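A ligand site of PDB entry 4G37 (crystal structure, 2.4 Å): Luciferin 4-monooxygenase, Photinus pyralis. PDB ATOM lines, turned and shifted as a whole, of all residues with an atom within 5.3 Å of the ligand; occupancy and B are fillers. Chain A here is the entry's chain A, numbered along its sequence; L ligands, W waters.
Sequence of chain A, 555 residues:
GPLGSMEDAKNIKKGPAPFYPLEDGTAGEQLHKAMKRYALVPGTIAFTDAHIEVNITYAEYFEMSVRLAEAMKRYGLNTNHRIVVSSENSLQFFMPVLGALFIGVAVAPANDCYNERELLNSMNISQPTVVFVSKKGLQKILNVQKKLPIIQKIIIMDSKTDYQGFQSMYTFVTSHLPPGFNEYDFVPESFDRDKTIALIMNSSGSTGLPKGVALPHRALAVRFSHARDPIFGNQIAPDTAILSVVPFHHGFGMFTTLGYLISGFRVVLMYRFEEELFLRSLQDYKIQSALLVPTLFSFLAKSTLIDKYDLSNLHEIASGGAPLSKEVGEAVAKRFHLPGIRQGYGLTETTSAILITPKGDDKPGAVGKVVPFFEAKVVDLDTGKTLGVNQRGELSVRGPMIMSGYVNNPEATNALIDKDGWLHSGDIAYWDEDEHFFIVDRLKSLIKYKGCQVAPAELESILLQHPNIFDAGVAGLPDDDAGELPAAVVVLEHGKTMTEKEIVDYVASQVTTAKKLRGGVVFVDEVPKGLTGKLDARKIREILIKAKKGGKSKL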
ATOM      1  N   ARG A 223       8.346  20.129  27.165  1.00  0.00           N
ATOM      2  CA  ARG A 223       8.871  21.469  27.405  1.00  0.00           C
ATOM      3  C   ARG A 223       7.783  22.411  27.927  1.00  0.00           C
ATOM      4  O   ARG A 223       8.025  23.185  28.860  1.00  0.00           O
ATOM      5  CB  ARG A 223       9.518  22.046  26.134  1.00  0.00           C
ATOM      6  CG  ARG A 223       9.869  23.533  26.261  1.00  0.00           C
ATOM      7  CD  ARG A 223      10.873  23.756  27.382  1.00  0.00           C
ATOM      8  NE  ARG A 223      10.984  25.159  27.764  1.00  0.00           N
ATOM      9  CZ  ARG A 223      11.563  25.585  28.901  1.00  0.00           C
ATOM     10  NH1 ARG A 223      12.089  24.699  29.751  1.00  0.00           N
ATOM     11  NH2 ARG A 223      11.607  26.892  29.173  1.00  0.00           N
ATOM     12  N   HIS A 250      18.179  28.789  17.575  1.00  0.00           N
ATOM     13  CA  HIS A 250      18.816  27.735  18.376  1.00  0.00           C
ATOM     14  C   HIS A 250      17.856  27.251  19.468  1.00  0.00           C
ATOM     15  O   HIS A 250      16.895  27.944  19.776  1.00  0.00           O
ATOM     16  CB  HIS A 250      20.101  28.285  18.992  1.00  0.00           C
ATOM     17  CG  HIS A 250      20.804  27.312  19.887  1.00  0.00           C
ATOM     18  ND1 HIS A 250      20.548  27.233  21.245  1.00  0.00           N
ATOM     19  CD2 HIS A 250      21.746  26.379  19.615  1.00  0.00           C
ATOM     20  CE1 HIS A 250      21.299  26.288  21.767  1.00  0.00           C
ATOM     21  NE2 HIS A 250      22.040  25.756  20.812  1.00  0.00           N
ATOM     22  N   GLY A 251      18.105  26.069  20.025  1.00  0.00           N
ATOM     23  CA  GLY A 251      17.233  25.449  21.026  1.00  0.00           C
ATOM     24  C   GLY A 251      17.001  26.252  22.301  1.00  0.00           C
ATOM     25  O   GLY A 251      15.911  26.253  22.874  1.00  0.00           O
ATOM     26  N   PHE A 252      18.025  26.968  22.747  1.00  0.00           N
ATOM     27  CA  PHE A 252      17.908  27.847  23.909  1.00  0.00           C
ATOM     28  C   PHE A 252      16.843  28.910  23.670  1.00  0.00           C
ATOM     29  O   PHE A 252      15.975  29.110  24.506  1.00  0.00           O
ATOM     30  CB  PHE A 252      19.271  28.484  24.237  1.00  0.00           C
ATOM     31  CG  PHE A 252      19.290  29.293  25.503  1.00  0.00           C
ATOM     32  CD1 PHE A 252      18.285  29.198  26.438  1.00  0.00           C
ATOM     33  CD2 PHE A 252      20.332  30.157  25.758  1.00  0.00           C
ATOM     34  CE1 PHE A 252      18.316  29.967  27.606  1.00  0.00           C
ATOM     35  CE2 PHE A 252      20.386  30.917  26.909  1.00  0.00           C
ATOM     36  CZ  PHE A 252      19.372  30.819  27.830  1.00  0.00           C
ATOM     37  N   THR A 256      12.594  28.295  24.976  1.00  0.00           N
ATOM     38  CA  THR A 256      12.224  29.249  25.998  1.00  0.00           C
ATOM     39  C   THR A 256      11.079  30.123  25.503  1.00  0.00           C
ATOM     40  O   THR A 256      10.084  30.309  26.223  1.00  0.00           O
ATOM     41  CB  THR A 256      13.418  30.092  26.477  1.00  0.00           C
ATOM     42  OG1 THR A 256      14.052  30.719  25.362  1.00  0.00           O
ATOM     43  CG2 THR A 256      14.410  29.201  27.178  1.00  0.00           C
ATOM     44  N   LEU A 291      16.140  36.619  30.524  1.00  0.00           N
ATOM     45  CA  LEU A 291      16.793  35.425  30.012  1.00  0.00           C
ATOM     46  C   LEU A 291      18.060  35.845  29.251  1.00  0.00           C
ATOM     47  O   LEU A 291      17.992  36.428  28.175  1.00  0.00           O
ATOM     48  CB  LEU A 291      15.834  34.648  29.105  1.00  0.00           C
ATOM     49  CG  LEU A 291      16.357  33.308  28.588  1.00  0.00           C
ATOM     50  CD1 LEU A 291      16.464  32.317  29.734  1.00  0.00           C
ATOM     51  CD2 LEU A 291      15.492  32.783  27.440  1.00  0.00           C
ATOM     52  N   ALA A 318      17.911  34.449  34.540  1.00  0.00           N
ATOM     53  CA  ALA A 318      18.350  33.115  34.107  1.00  0.00           C
ATOM     54  C   ALA A 318      19.495  33.164  33.072  1.00  0.00           C
ATOM     55  O   ALA A 318      19.685  34.157  32.375  1.00  0.00           O
ATOM     56  CB  ALA A 318      17.186  32.296  33.579  1.00  0.00           C
ATOM     57  N   SER A 319      20.268  32.081  32.992  1.00  0.00           N
ATOM     58  CA  SER A 319      21.327  31.923  32.004  1.00  0.00           C
ATOM     59  C   SER A 319      21.443  30.455  31.581  1.00  0.00           C
ATOM     60  O   SER A 319      20.988  29.549  32.282  1.00  0.00           O
ATOM     61  CB  SER A 319      22.666  32.421  32.556  1.00  0.00           C
ATOM     62  OG  SER A 319      23.740  32.092  31.685  1.00  0.00           O
ATOM     63  N   GLY A 320      22.063  30.210  30.434  1.00  0.00           N
ATOM     64  CA  GLY A 320      22.166  28.859  29.945  1.00  0.00           C
ATOM     65  C   GLY A 320      22.926  28.834  28.641  1.00  0.00           C
ATOM     66  O   GLY A 320      23.285  29.880  28.108  1.00  0.00           O
ATOM     67  N   GLY A 321      23.194  27.626  28.145  1.00  0.00           N
ATOM     68  CA  GLY A 321      23.865  27.477  26.869  1.00  0.00           C
ATOM     69  C   GLY A 321      25.375  27.458  27.003  1.00  0.00           C
ATOM     70  O   GLY A 321      26.066  27.007  26.091  1.00  0.00           O
ATOM     71  N   ALA A 322      25.898  27.916  28.143  1.00  0.00           N
ATOM     72  CA  ALA A 322      27.345  27.952  28.339  1.00  0.00           C
ATOM     73  C   ALA A 322      27.727  28.187  29.811  1.00  0.00           C
ATOM     74  O   ALA A 322      26.874  28.584  30.616  1.00  0.00           O
ATOM     75  CB  ALA A 322      28.004  29.011  27.394  1.00  0.00           C
ATOM     76  N   PRO A 323      28.988  27.925  30.167  1.00  0.00           N
ATOM     77  CA  PRO A 323      29.283  28.026  31.610  1.00  0.00           C
ATOM     78  C   PRO A 323      29.185  29.445  32.201  1.00  0.00           C
ATOM     79  O   PRO A 323      29.615  30.424  31.604  1.00  0.00           O
ATOM     80  CB  PRO A 323      30.705  27.451  31.755  1.00  0.00           C
ATOM     81  CG  PRO A 323      31.201  27.165  30.363  1.00  0.00           C
ATOM     82  CD  PRO A 323      30.026  27.194  29.419  1.00  0.00           C
ATOM     83  N   LEU A 324      28.559  29.509  33.365  1.00  0.00           N
ATOM     84  CA  LEU A 324      28.498  30.720  34.156  1.00  0.00           C
ATOM     85  C   LEU A 324      29.493  30.584  35.301  1.00  0.00           C
ATOM     86  O   LEU A 324      29.489  29.578  36.016  1.00  0.00           O
ATOM     87  CB  LEU A 324      27.100  30.914  34.737  1.00  0.00           C
ATOM     88  CG  LEU A 324      26.945  32.099  35.698  1.00  0.00           C
ATOM     89  CD1 LEU A 324      27.090  33.413  34.933  1.00  0.00           C
ATOM     90  CD2 LEU A 324      25.606  32.061  36.447  1.00  0.00           C
ATOM     91  N   ARG A 342      19.459  31.910  38.081  1.00  0.00           N
ATOM     92  CA  ARG A 342      18.688  30.748  37.713  1.00  0.00           C
ATOM     93  C   ARG A 342      19.340  30.150  36.474  1.00  0.00           C
ATOM     94  O   ARG A 342      19.815  30.878  35.602  1.00  0.00           O
ATOM     95  CB  ARG A 342      17.253  31.212  37.439  1.00  0.00           C
ATOM     96  CG  ARG A 342      16.211  30.119  37.375  1.00  0.00           C
ATOM     97  CD  ARG A 342      15.079  30.349  38.360  1.00  0.00           C
ATOM     98  NE  ARG A 342      14.420  29.074  38.604  1.00  0.00           N
ATOM     99  CZ  ARG A 342      13.447  28.574  37.836  1.00  0.00           C
ATOM    100  NH1 ARG A 342      13.003  29.256  36.794  1.00  0.00           N
ATOM    101  NH2 ARG A 342      12.925  27.396  38.126  1.00  0.00           N
ATOM    102  N   GLN A 343      19.420  28.825  36.373  1.00  0.00           N
ATOM    103  CA  GLN A 343      20.146  28.262  35.226  1.00  0.00           C
ATOM    104  C   GLN A 343      19.498  27.054  34.609  1.00  0.00           C
ATOM    105  O   GLN A 343      18.718  26.330  35.243  1.00  0.00           O
ATOM    106  CB  GLN A 343      21.570  27.855  35.614  1.00  0.00           C
ATOM    107  CG  GLN A 343      22.587  28.946  35.558  1.00  0.00           C
ATOM    108  CD  GLN A 343      23.987  28.394  35.604  1.00  0.00           C
ATOM    109  OE1 GLN A 343      24.535  27.942  34.575  1.00  0.00           O
ATOM    110  NE2 GLN A 343      24.584  28.407  36.803  1.00  0.00           N
ATOM    111  N   GLY A 344      19.895  26.808  33.361  1.00  0.00           N
ATOM    112  CA  GLY A 344      19.458  25.660  32.616  1.00  0.00           C
ATOM    113  C   GLY A 344      20.577  25.133  31.752  1.00  0.00           C
ATOM    114  O   GLY A 344      21.365  25.897  31.177  1.00  0.00           O
ATOM    115  N   TYR A 345      20.670  23.813  31.689  1.00  0.00           N
ATOM    116  CA  TYR A 345      21.696  23.180  30.891  1.00  0.00           C
ATOM    117  C   TYR A 345      20.980  22.249  29.941  1.00  0.00           C
ATOM    118  O   TYR A 345      20.080  21.502  30.337  1.00  0.00           O
ATOM    119  CB  TYR A 345      22.630  22.373  31.798  1.00  0.00           C
ATOM    120  CG  TYR A 345      23.319  21.213  31.099  1.00  0.00           C
ATOM    121  CD1 TYR A 345      24.570  21.379  30.516  1.00  0.00           C
ATOM    122  CD2 TYR A 345      22.727  19.953  31.050  1.00  0.00           C
ATOM    123  CE1 TYR A 345      25.217  20.320  29.890  1.00  0.00           C
ATOM    124  CE2 TYR A 345      23.357  18.893  30.407  1.00  0.00           C
ATOM    125  CZ  TYR A 345      24.600  19.078  29.838  1.00  0.00           C
ATOM    126  OH  TYR A 345      25.229  18.024  29.208  1.00  0.00           O
ATOM    127  N   GLY A 346      21.371  22.277  28.669  1.00  0.00           N
ATOM    128  CA  GLY A 346      20.766  21.383  27.704  1.00  0.00           C
ATOM    129  C   GLY A 346      21.536  21.304  26.419  1.00  0.00           C
ATOM    130  O   GLY A 346      22.501  22.049  26.188  1.00  0.00           O
ATOM    131  N   LEU A 347      21.095  20.399  25.562  1.00  0.00           N
ATOM    132  CA  LEU A 347      21.685  20.278  24.256  1.00  0.00           C
ATOM    133  C   LEU A 347      20.552  20.352  23.286  1.00  0.00           C
ATOM    134  O   LEU A 347      19.394  20.126  23.638  1.00  0.00           O
ATOM    135  CB  LEU A 347      22.408  18.931  24.095  1.00  0.00           C
ATOM    136  CG  LEU A 347      23.531  18.576  25.060  1.00  0.00           C
ATOM    137  CD1 LEU A 347      23.009  17.776  26.247  1.00  0.00           C
ATOM    138  CD2 LEU A 347      24.611  17.801  24.345  1.00  0.00           C
ATOM    139  N   THR A 348      20.892  20.654  22.040  1.00  0.00           N
ATOM    140  CA  THR A 348      19.926  20.708  20.978  1.00  0.00           C
ATOM    141  C   THR A 348      19.179  19.391  20.878  1.00  0.00           C
ATOM    142  O   THR A 348      17.981  19.378  20.577  1.00  0.00           O
ATOM    143  CB  THR A 348      20.613  20.961  19.616  1.00  0.00           C
ATOM    144  OG1 THR A 348      21.401  22.154  19.702  1.00  0.00           O
ATOM    145  CG2 THR A 348      19.576  21.100  18.513  1.00  0.00           C
ATOM    146  N   GLU A 349      19.902  18.294  21.108  1.00  0.00           N
ATOM    147  CA  GLU A 349      19.351  16.940  20.999  1.00  0.00           C
ATOM    148  C   GLU A 349      18.407  16.593  22.151  1.00  0.00           C
ATOM    149  O   GLU A 349      17.689  15.600  22.078  1.00  0.00           O
ATOM    150  CB  GLU A 349      20.482  15.910  20.928  1.00  0.00           C
ATOM    151  CG  GLU A 349      21.208  15.844  19.577  1.00  0.00           C
ATOM    152  CD  GLU A 349      22.320  16.875  19.457  1.00  0.00           C
ATOM    153  OE1 GLU A 349      22.504  17.679  20.402  1.00  0.00           O
ATOM    154  OE2 GLU A 349      23.019  16.868  18.415  1.00  0.00           O
ATOM    155  N   THR A 351      16.108  18.750  23.120  1.00  0.00           N
ATOM    156  CA  THR A 351      15.120  19.815  22.919  1.00  0.00           C
ATOM    157  C   THR A 351      15.458  21.070  23.720  1.00  0.00           C
ATOM    158  O   THR A 351      15.828  22.101  23.164  1.00  0.00           O
ATOM    159  CB  THR A 351      13.658  19.361  23.258  1.00  0.00           C
ATOM    160  OG1 THR A 351      13.299  18.223  22.476  1.00  0.00           O
ATOM    161  CG2 THR A 351      12.640  20.466  22.971  1.00  0.00           C
ATOM    162  N   SER A 352      15.297  20.995  25.046  1.00  0.00           N
ATOM    163  CA  SER A 352      15.521  22.159  25.888  1.00  0.00           C
ATOM    164  C   SER A 352      16.382  21.769  27.082  1.00  0.00           C
ATOM    165  O   SER A 352      16.968  20.685  27.102  1.00  0.00           O
ATOM    166  CB  SER A 352      14.178  22.717  26.352  1.00  0.00           C
ATOM    167  OG  SER A 352      14.348  23.950  27.021  1.00  0.00           O
ATOM    168  N   ALA A 353      16.433  22.650  28.094  1.00  0.00           N
ATOM    169  CA  ALA A 353      17.180  22.328  29.314  1.00  0.00           C
ATOM    170  C   ALA A 353      16.615  21.074  29.984  1.00  0.00           C
ATOM    171  O   ALA A 353      15.408  20.867  30.038  1.00  0.00           O
ATOM    172  CB  ALA A 353      17.176  23.522  30.285  1.00  0.00           C
ATOM    173  N   ILE A 356      17.905  22.105  35.520  1.00  0.00           N
ATOM    174  CA  ILE A 356      17.427  23.469  35.761  1.00  0.00           C
ATOM    175  C   ILE A 356      17.454  23.751  37.246  1.00  0.00           C
ATOM    176  O   ILE A 356      17.083  22.878  38.041  1.00  0.00           O
ATOM    177  CB  ILE A 356      15.979  23.666  35.252  1.00  0.00           C
ATOM    178  CG1 ILE A 356      15.899  23.464  33.730  1.00  0.00           C
ATOM    179  CG2 ILE A 356      15.428  25.064  35.611  1.00  0.00           C
ATOM    180  CD1 ILE A 356      14.503  23.656  33.182  1.00  0.00           C
ATOM    181  N   VAL A 367      24.362  23.965  37.980  1.00  0.00           N
ATOM    182  CA  VAL A 367      23.484  24.254  36.858  1.00  0.00           C
ATOM    183  C   VAL A 367      22.058  23.733  37.100  1.00  0.00           C
ATOM    184  O   VAL A 367      21.177  23.972  36.271  1.00  0.00           O
ATOM    185  CB  VAL A 367      24.027  23.689  35.537  1.00  0.00           C
ATOM    186  CG1 VAL A 367      25.384  24.289  35.241  1.00  0.00           C
ATOM    187  CG2 VAL A 367      24.075  22.170  35.583  1.00  0.00           C
ATOM    188  N   SER A 425      26.473  13.062  26.720  1.00  0.00           N
ATOM    189  CA  SER A 425      26.429  14.461  26.338  1.00  0.00           C
ATOM    190  C   SER A 425      27.755  15.086  25.940  1.00  0.00           C
ATOM    191  O   SER A 425      27.788  16.213  25.430  1.00  0.00           O
ATOM    192  CB  SER A 425      25.867  15.282  27.492  1.00  0.00           C
ATOM    193  OG  SER A 425      26.788  15.286  28.546  1.00  0.00           O
ATOM    194  N   ASP A 427      29.787  16.109  28.066  1.00  0.00           N
ATOM    195  CA  ASP A 427      30.167  16.990  29.182  1.00  0.00           C
ATOM    196  C   ASP A 427      30.590  16.239  30.438  1.00  0.00           C
ATOM    197  O   ASP A 427      30.164  15.113  30.712  1.00  0.00           O
ATOM    198  CB  ASP A 427      29.031  17.934  29.555  1.00  0.00           C
ATOM    199  CG  ASP A 427      28.629  18.826  28.429  1.00  0.00           C
ATOM    200  OD1 ASP A 427      29.456  19.708  28.062  1.00  0.00           O
ATOM    201  OD2 ASP A 427      27.497  18.650  27.922  1.00  0.00           O
ATOM    202  N   ILE A 439      28.612  21.285  36.141  1.00  0.00           N
ATOM    203  CA  ILE A 439      29.338  21.025  34.893  1.00  0.00           C
ATOM    204  C   ILE A 439      30.749  21.570  35.042  1.00  0.00           C
ATOM    205  O   ILE A 439      30.937  22.788  35.103  1.00  0.00           O
ATOM    206  CB  ILE A 439      28.666  21.738  33.725  1.00  0.00           C
ATOM    207  CG1 ILE A 439      27.186  21.351  33.659  1.00  0.00           C
ATOM    208  CG2 ILE A 439      29.399  21.447  32.414  1.00  0.00           C
ATOM    209  CD1 ILE A 439      26.936  19.920  33.197  1.00  0.00           C
ATOM    210  N   ARG A 442      34.520  19.717  29.680  1.00  0.00           N
ATOM    211  CA  ARG A 442      33.938  19.260  28.432  1.00  0.00           C
ATOM    212  C   ARG A 442      34.855  18.200  27.801  1.00  0.00           C
ATOM    213  O   ARG A 442      36.054  18.424  27.628  1.00  0.00           O
ATOM    214  CB  ARG A 442      33.743  20.443  27.484  1.00  0.00           C
ATOM    215  CG  ARG A 442      32.989  20.107  26.214  1.00  0.00           C
ATOM    216  CD  ARG A 442      32.673  21.367  25.415  1.00  0.00           C
ATOM    217  NE  ARG A 442      32.190  22.427  26.286  1.00  0.00           N
ATOM    218  CZ  ARG A 442      32.169  23.722  25.988  1.00  0.00           C
ATOM    219  NH1 ARG A 442      32.601  24.158  24.797  1.00  0.00           N
ATOM    220  NH2 ARG A 442      31.705  24.589  26.893  1.00  0.00           N
ATOM    221  N   LYS A 444      33.991  16.457  24.720  1.00  0.00           N
ATOM    222  CA  LYS A 444      33.888  16.666  23.279  1.00  0.00           C
ATOM    223  C   LYS A 444      34.636  17.911  22.813  1.00  0.00           C
ATOM    224  O   LYS A 444      34.905  18.834  23.604  1.00  0.00           O
ATOM    225  CB  LYS A 444      32.427  16.754  22.862  1.00  0.00           C
ATOM    226  CG  LYS A 444      31.657  17.882  23.545  1.00  0.00           C
ATOM    227  CD  LYS A 444      30.149  17.721  23.310  1.00  0.00           C
ATOM    228  CE  LYS A 444      29.333  18.884  23.876  1.00  0.00           C
ATOM    229  NZ  LYS A 444      27.894  18.482  24.018  1.00  0.00           N
ATOM    230  N   LEU A 446      34.232  21.076  21.014  1.00  0.00           N
ATOM    231  CA  LEU A 446      33.159  21.980  20.654  1.00  0.00           C
ATOM    232  C   LEU A 446      33.485  23.294  21.315  1.00  0.00           C
ATOM    233  O   LEU A 446      33.847  23.331  22.495  1.00  0.00           O
ATOM    234  CB  LEU A 446      31.818  21.458  21.158  1.00  0.00           C
ATOM    235  CG  LEU A 446      30.773  22.541  21.464  1.00  0.00           C
ATOM    236  CD1 LEU A 446      29.910  22.901  20.238  1.00  0.00           C
ATOM    237  CD2 LEU A 446      29.910  22.154  22.676  1.00  0.00           C
ATOM    238  N   LYS A 448      32.279  27.384  21.972  1.00  0.00           N
ATOM    239  CA  LYS A 448      31.215  28.364  21.884  1.00  0.00           C
ATOM    240  C   LYS A 448      31.800  29.758  22.040  1.00  0.00           C
ATOM    241  O   LYS A 448      32.159  30.177  23.143  1.00  0.00           O
ATOM    242  CB  LYS A 448      30.137  28.113  22.921  1.00  0.00           C
ATOM    243  CG  LYS A 448      29.307  26.881  22.653  1.00  0.00           C
ATOM    244  CD  LYS A 448      27.917  27.097  23.145  1.00  0.00           C
ATOM    245  CE  LYS A 448      27.134  25.815  23.144  1.00  0.00           C
ATOM    246  NZ  LYS A 448      25.730  26.101  23.521  1.00  0.00           N
ATOM    247  N   GLN A 453      28.311  28.261  18.011  1.00  0.00           N
ATOM    248  CA  GLN A 453      29.046  27.003  17.950  1.00  0.00           C
ATOM    249  C   GLN A 453      30.158  27.034  16.898  1.00  0.00           C
ATOM    250  O   GLN A 453      29.932  27.442  15.765  1.00  0.00           O
ATOM    251  CB  GLN A 453      28.108  25.840  17.645  1.00  0.00           C
ATOM    252  CG  GLN A 453      27.014  25.646  18.684  1.00  0.00           C
ATOM    253  CD  GLN A 453      26.140  24.460  18.349  1.00  0.00           C
ATOM    254  OE1 GLN A 453      26.634  23.368  18.080  1.00  0.00           O
ATOM    255  NE2 GLN A 453      24.821  24.682  18.348  1.00  0.00           N
HETATM  256  O1  LIG L   1      23.284  25.001  24.547  1.00  0.00           O
HETATM  257  C1  LIG L   1      22.365  24.305  24.134  1.00  0.00           C
HETATM  258  C2  LIG L   1      20.971  24.365  24.663  1.00  0.00           C
HETATM  259  N1  LIG L   1      20.665  25.082  25.696  1.00  0.00           N
HETATM  260  C3  LIG L   1      19.999  23.652  24.015  1.00  0.00           C
HETATM  261  S1  LIG L   1      18.574  24.035  24.937  1.00  0.00           S
HETATM  262  C4  LIG L   1      19.382  25.087  26.058  1.00  0.00           C
HETATM  263  C5  LIG L   1      18.869  25.763  27.138  1.00  0.00           C
HETATM  264  S2  LIG L   1      19.846  26.526  28.347  1.00  0.00           S
HETATM  265  C6  LIG L   1      18.473  27.085  29.321  1.00  0.00           C
HETATM  266  C7  LIG L   1      18.368  27.843  30.504  1.00  0.00           C
HETATM  267  C8  LIG L   1      17.098  28.116  31.012  1.00  0.00           C
HETATM  268  O2  LIG L   1      16.964  28.856  32.201  1.00  0.00           O
HETATM  269  C9  LIG L   1      17.366  26.614  28.605  1.00  0.00           C
HETATM  270  N2  LIG L   1      17.633  25.955  27.499  1.00  0.00           N
HETATM  271  C10 LIG L   1      16.076  26.920  29.150  1.00  0.00           C
HETATM  272  C11 LIG L   1      15.979  27.666  30.331  1.00  0.00           C
HETATM  273  N3  LIG L   1      22.550  23.341  23.068  1.00  0.00           N
HETATM  274  S3  LIG L   1      23.997  23.164  22.309  1.00  0.00           S
HETATM  275  O3  LIG L   1      24.198  24.346  21.543  1.00  0.00           O
HETATM  276  O4  LIG L   1      23.860  22.062  21.373  1.00  0.00           O
HETATM  277  O5  LIG L   1      25.176  22.963  23.243  1.00  0.00           O
HETATM  278  C12 LIG L   1      25.109  22.047  24.319  1.00  0.00           C
HETATM  279  C13 LIG L   1      26.335  22.232  25.195  1.00  0.00           C
HETATM  280  C14 LIG L   1      26.358  21.358  26.394  1.00  0.00           C
HETATM  281  O6  LIG L   1      26.732  20.073  26.065  1.00  0.00           O
HETATM  282  C15 LIG L   1      27.371  22.046  27.192  1.00  0.00           C
HETATM  283  O7  LIG L   1      28.642  21.804  26.716  1.00  0.00           O
HETATM  284  C16 LIG L   1      27.038  23.464  26.914  1.00  0.00           C
HETATM  285  O8  LIG L   1      26.405  23.560  25.649  1.00  0.00           O
HETATM  286  N4  LIG L   1      26.175  24.044  27.896  1.00  0.00           N
HETATM  287  C17 LIG L   1      26.510  24.432  29.146  1.00  0.00           C
HETATM  288  N5  LIG L   1      27.644  24.402  29.866  1.00  0.00           N
HETATM  289  C18 LIG L   1      27.661  24.871  31.108  1.00  0.00           C
HETATM  290  N6  LIG L   1      26.573  25.361  31.717  1.00  0.00           N
HETATM  291  C19 LIG L   1      25.340  24.957  29.738  1.00  0.00           C
HETATM  292  C20 LIG L   1      25.405  25.445  31.070  1.00  0.00           C
HETATM  293  N7  LIG L   1      24.257  25.993  31.732  1.00  0.00           N
HETATM  294  N8  LIG L   1      24.377  24.862  28.828  1.00  0.00           N
HETATM  295  C21 LIG L   1      24.865  24.323  27.717  1.00  0.00           C
HETATM  296  O   HOH W   1      15.444  25.756  25.507  1.00  0.00           O
HETATM  297  O   HOH W   2      27.447  26.612  34.155  1.00  0.00           O
HETATM  298  O   HOH W   3      24.717  29.353  31.971  1.00  0.00           O
HETATM  299  O   HOH W   4      30.385  23.479  29.340  1.00  0.00           O
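N7 of the ligand is in hydrogen-bond range of OE1 of Gln 343 (3.5 Å). N of Thr 348 lies within hydrogen-bond range of N3 of the ligand, 3.3 Å away. The side-chain carboxylate of Asp 427 is in hydrogen-bond range of an oxygen (O6) of the ligand (2.5 Å). The side-chain amide nitrogen of Gln 453 is in hydrogen-bond range of an oxygen (O3) of the ligand (3.3 Å). N3 of the ligand sits close to O of Gly 346 (3.4 Å). OG1 of Thr 348 is in hydrogen-bond range of O4 of the ligand, at 3.0 Å. The backbone NH (N) of Ala 322 sits close to a nitrogen (N8) of the ligand (3.5 Å). N of Phe 252 lies close to S1 of the ligand, 3.7 Å away. A nitrogen (N8) of the ligand is in hydrogen-bond range of the backbone NH (N) of Gly 321, 3.1 Å away. A nitrogen (N7) of the ligand is in hydrogen-bond range of the backbone carbonyl oxygen of Gly 344, 2.9 Å away. An oxygen (O1) of the ligand is in hydrogen-bond range of the side-chain amino group of Lys 448, at 2.9 Å. A ring nitrogen (NE2) of His 250 lies within hydrogen-bond range of an oxygen (O3) of the ligand (2.7 Å). NZ of Lys 444 lies within hydrogen-bond range of O6 of the ligand (2.8 Å).
A ring nitrogen (ND1) of His 250 is in hydrogen-bond range of the backbone NH of Phe 252 (2.9 Å). The side-chain carboxylate (OD2) of Asp 427 lies within salt-bridge range of the side-chain amino group (NZ) of Lys 444 (3.9 Å). The guanidinium group of Arg 442 is in hydrogen-bond range of the backbone carbonyl oxygen of Leu 446, 2.7 Å away. The side-chain hydroxyl (OG1) of Thr 256 is in hydrogen-bond range of the backbone carbonyl oxygen (O) of Phe 252 (2.6 Å). OG of Ser 425 sits at hydrogen-bond distance from OH of Tyr 345 (3.2 Å). N of Ser 319 lies within hydrogen-bond range of O of Arg 342 (2.9 Å). O of Gly 321 lies within hydrogen-bond range of NZ of Lys 448 (2.7 Å). O of Ser 319 sits at hydrogen-bond distance from N of Gly 344 (3.1 Å).
A sulfur (S1) of the ligand lies close to the backbone carbonyl oxygen (O) of Thr 351 (3.8 Å). Residues that only touch the ligand: Leu 347, Thr 256, Pro 323, Ala 353, Ser 319, Arg 442, Gly 320, Ser 352, Ala 318, Tyr 345, Gly 251 and Val 367. Hydrophobic or aromatic side chains that line the ligand: His 250, Phe 252, Ala 318, Pro 323, Tyr 345, Leu 347, Ala 353 and Val 367. Within 4 Å of the ligand: His 250, Gly 251, Phe 252, Thr 256, Ala 318, Ser 319, Gly 320, Gly 321, Ala 322, Pro 323, Gln 343, Gly 344, Tyr 345, Gly 346, Leu 347, Thr 348, Thr 351, Ser 352, Ala 353, Val 367, Asp 427, Arg 442, Lys 444, Lys 448 and Gln 453.
Water W2 lies within hydrogen-bond range of a nitrogen (N6) of the ligand (2.9 Å), the backbone NH of Leu 324 (3.2 Å) and the side-chain amide oxygen of Gln 343 (3.2 Å). Water W4 lies within hydrogen-bond range of N5 of the ligand (2.9 Å) and NH2 of Arg 442 (3.0 Å). Water W1 lies within hydrogen-bond range of the side-chain hydroxyl (OG) of Ser 352, the backbone carbonyl oxygen (O) of Gly 251 and a nitrogen (N2) of the ligand. Water W3 lies within hydrogen-bond range of the backbone carbonyl oxygen (O) of Ala 322 (2.7 Å), the side-chain hydroxyl (OG) of Ser 319 (2.9 Å), the side-chain amide oxygen (OE1) of Gln 343 (3.0 Å), the backbone NH (N) of Gly 320 (3.2 Å) and a nitrogen (N7) of the ligand (3.4 Å).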
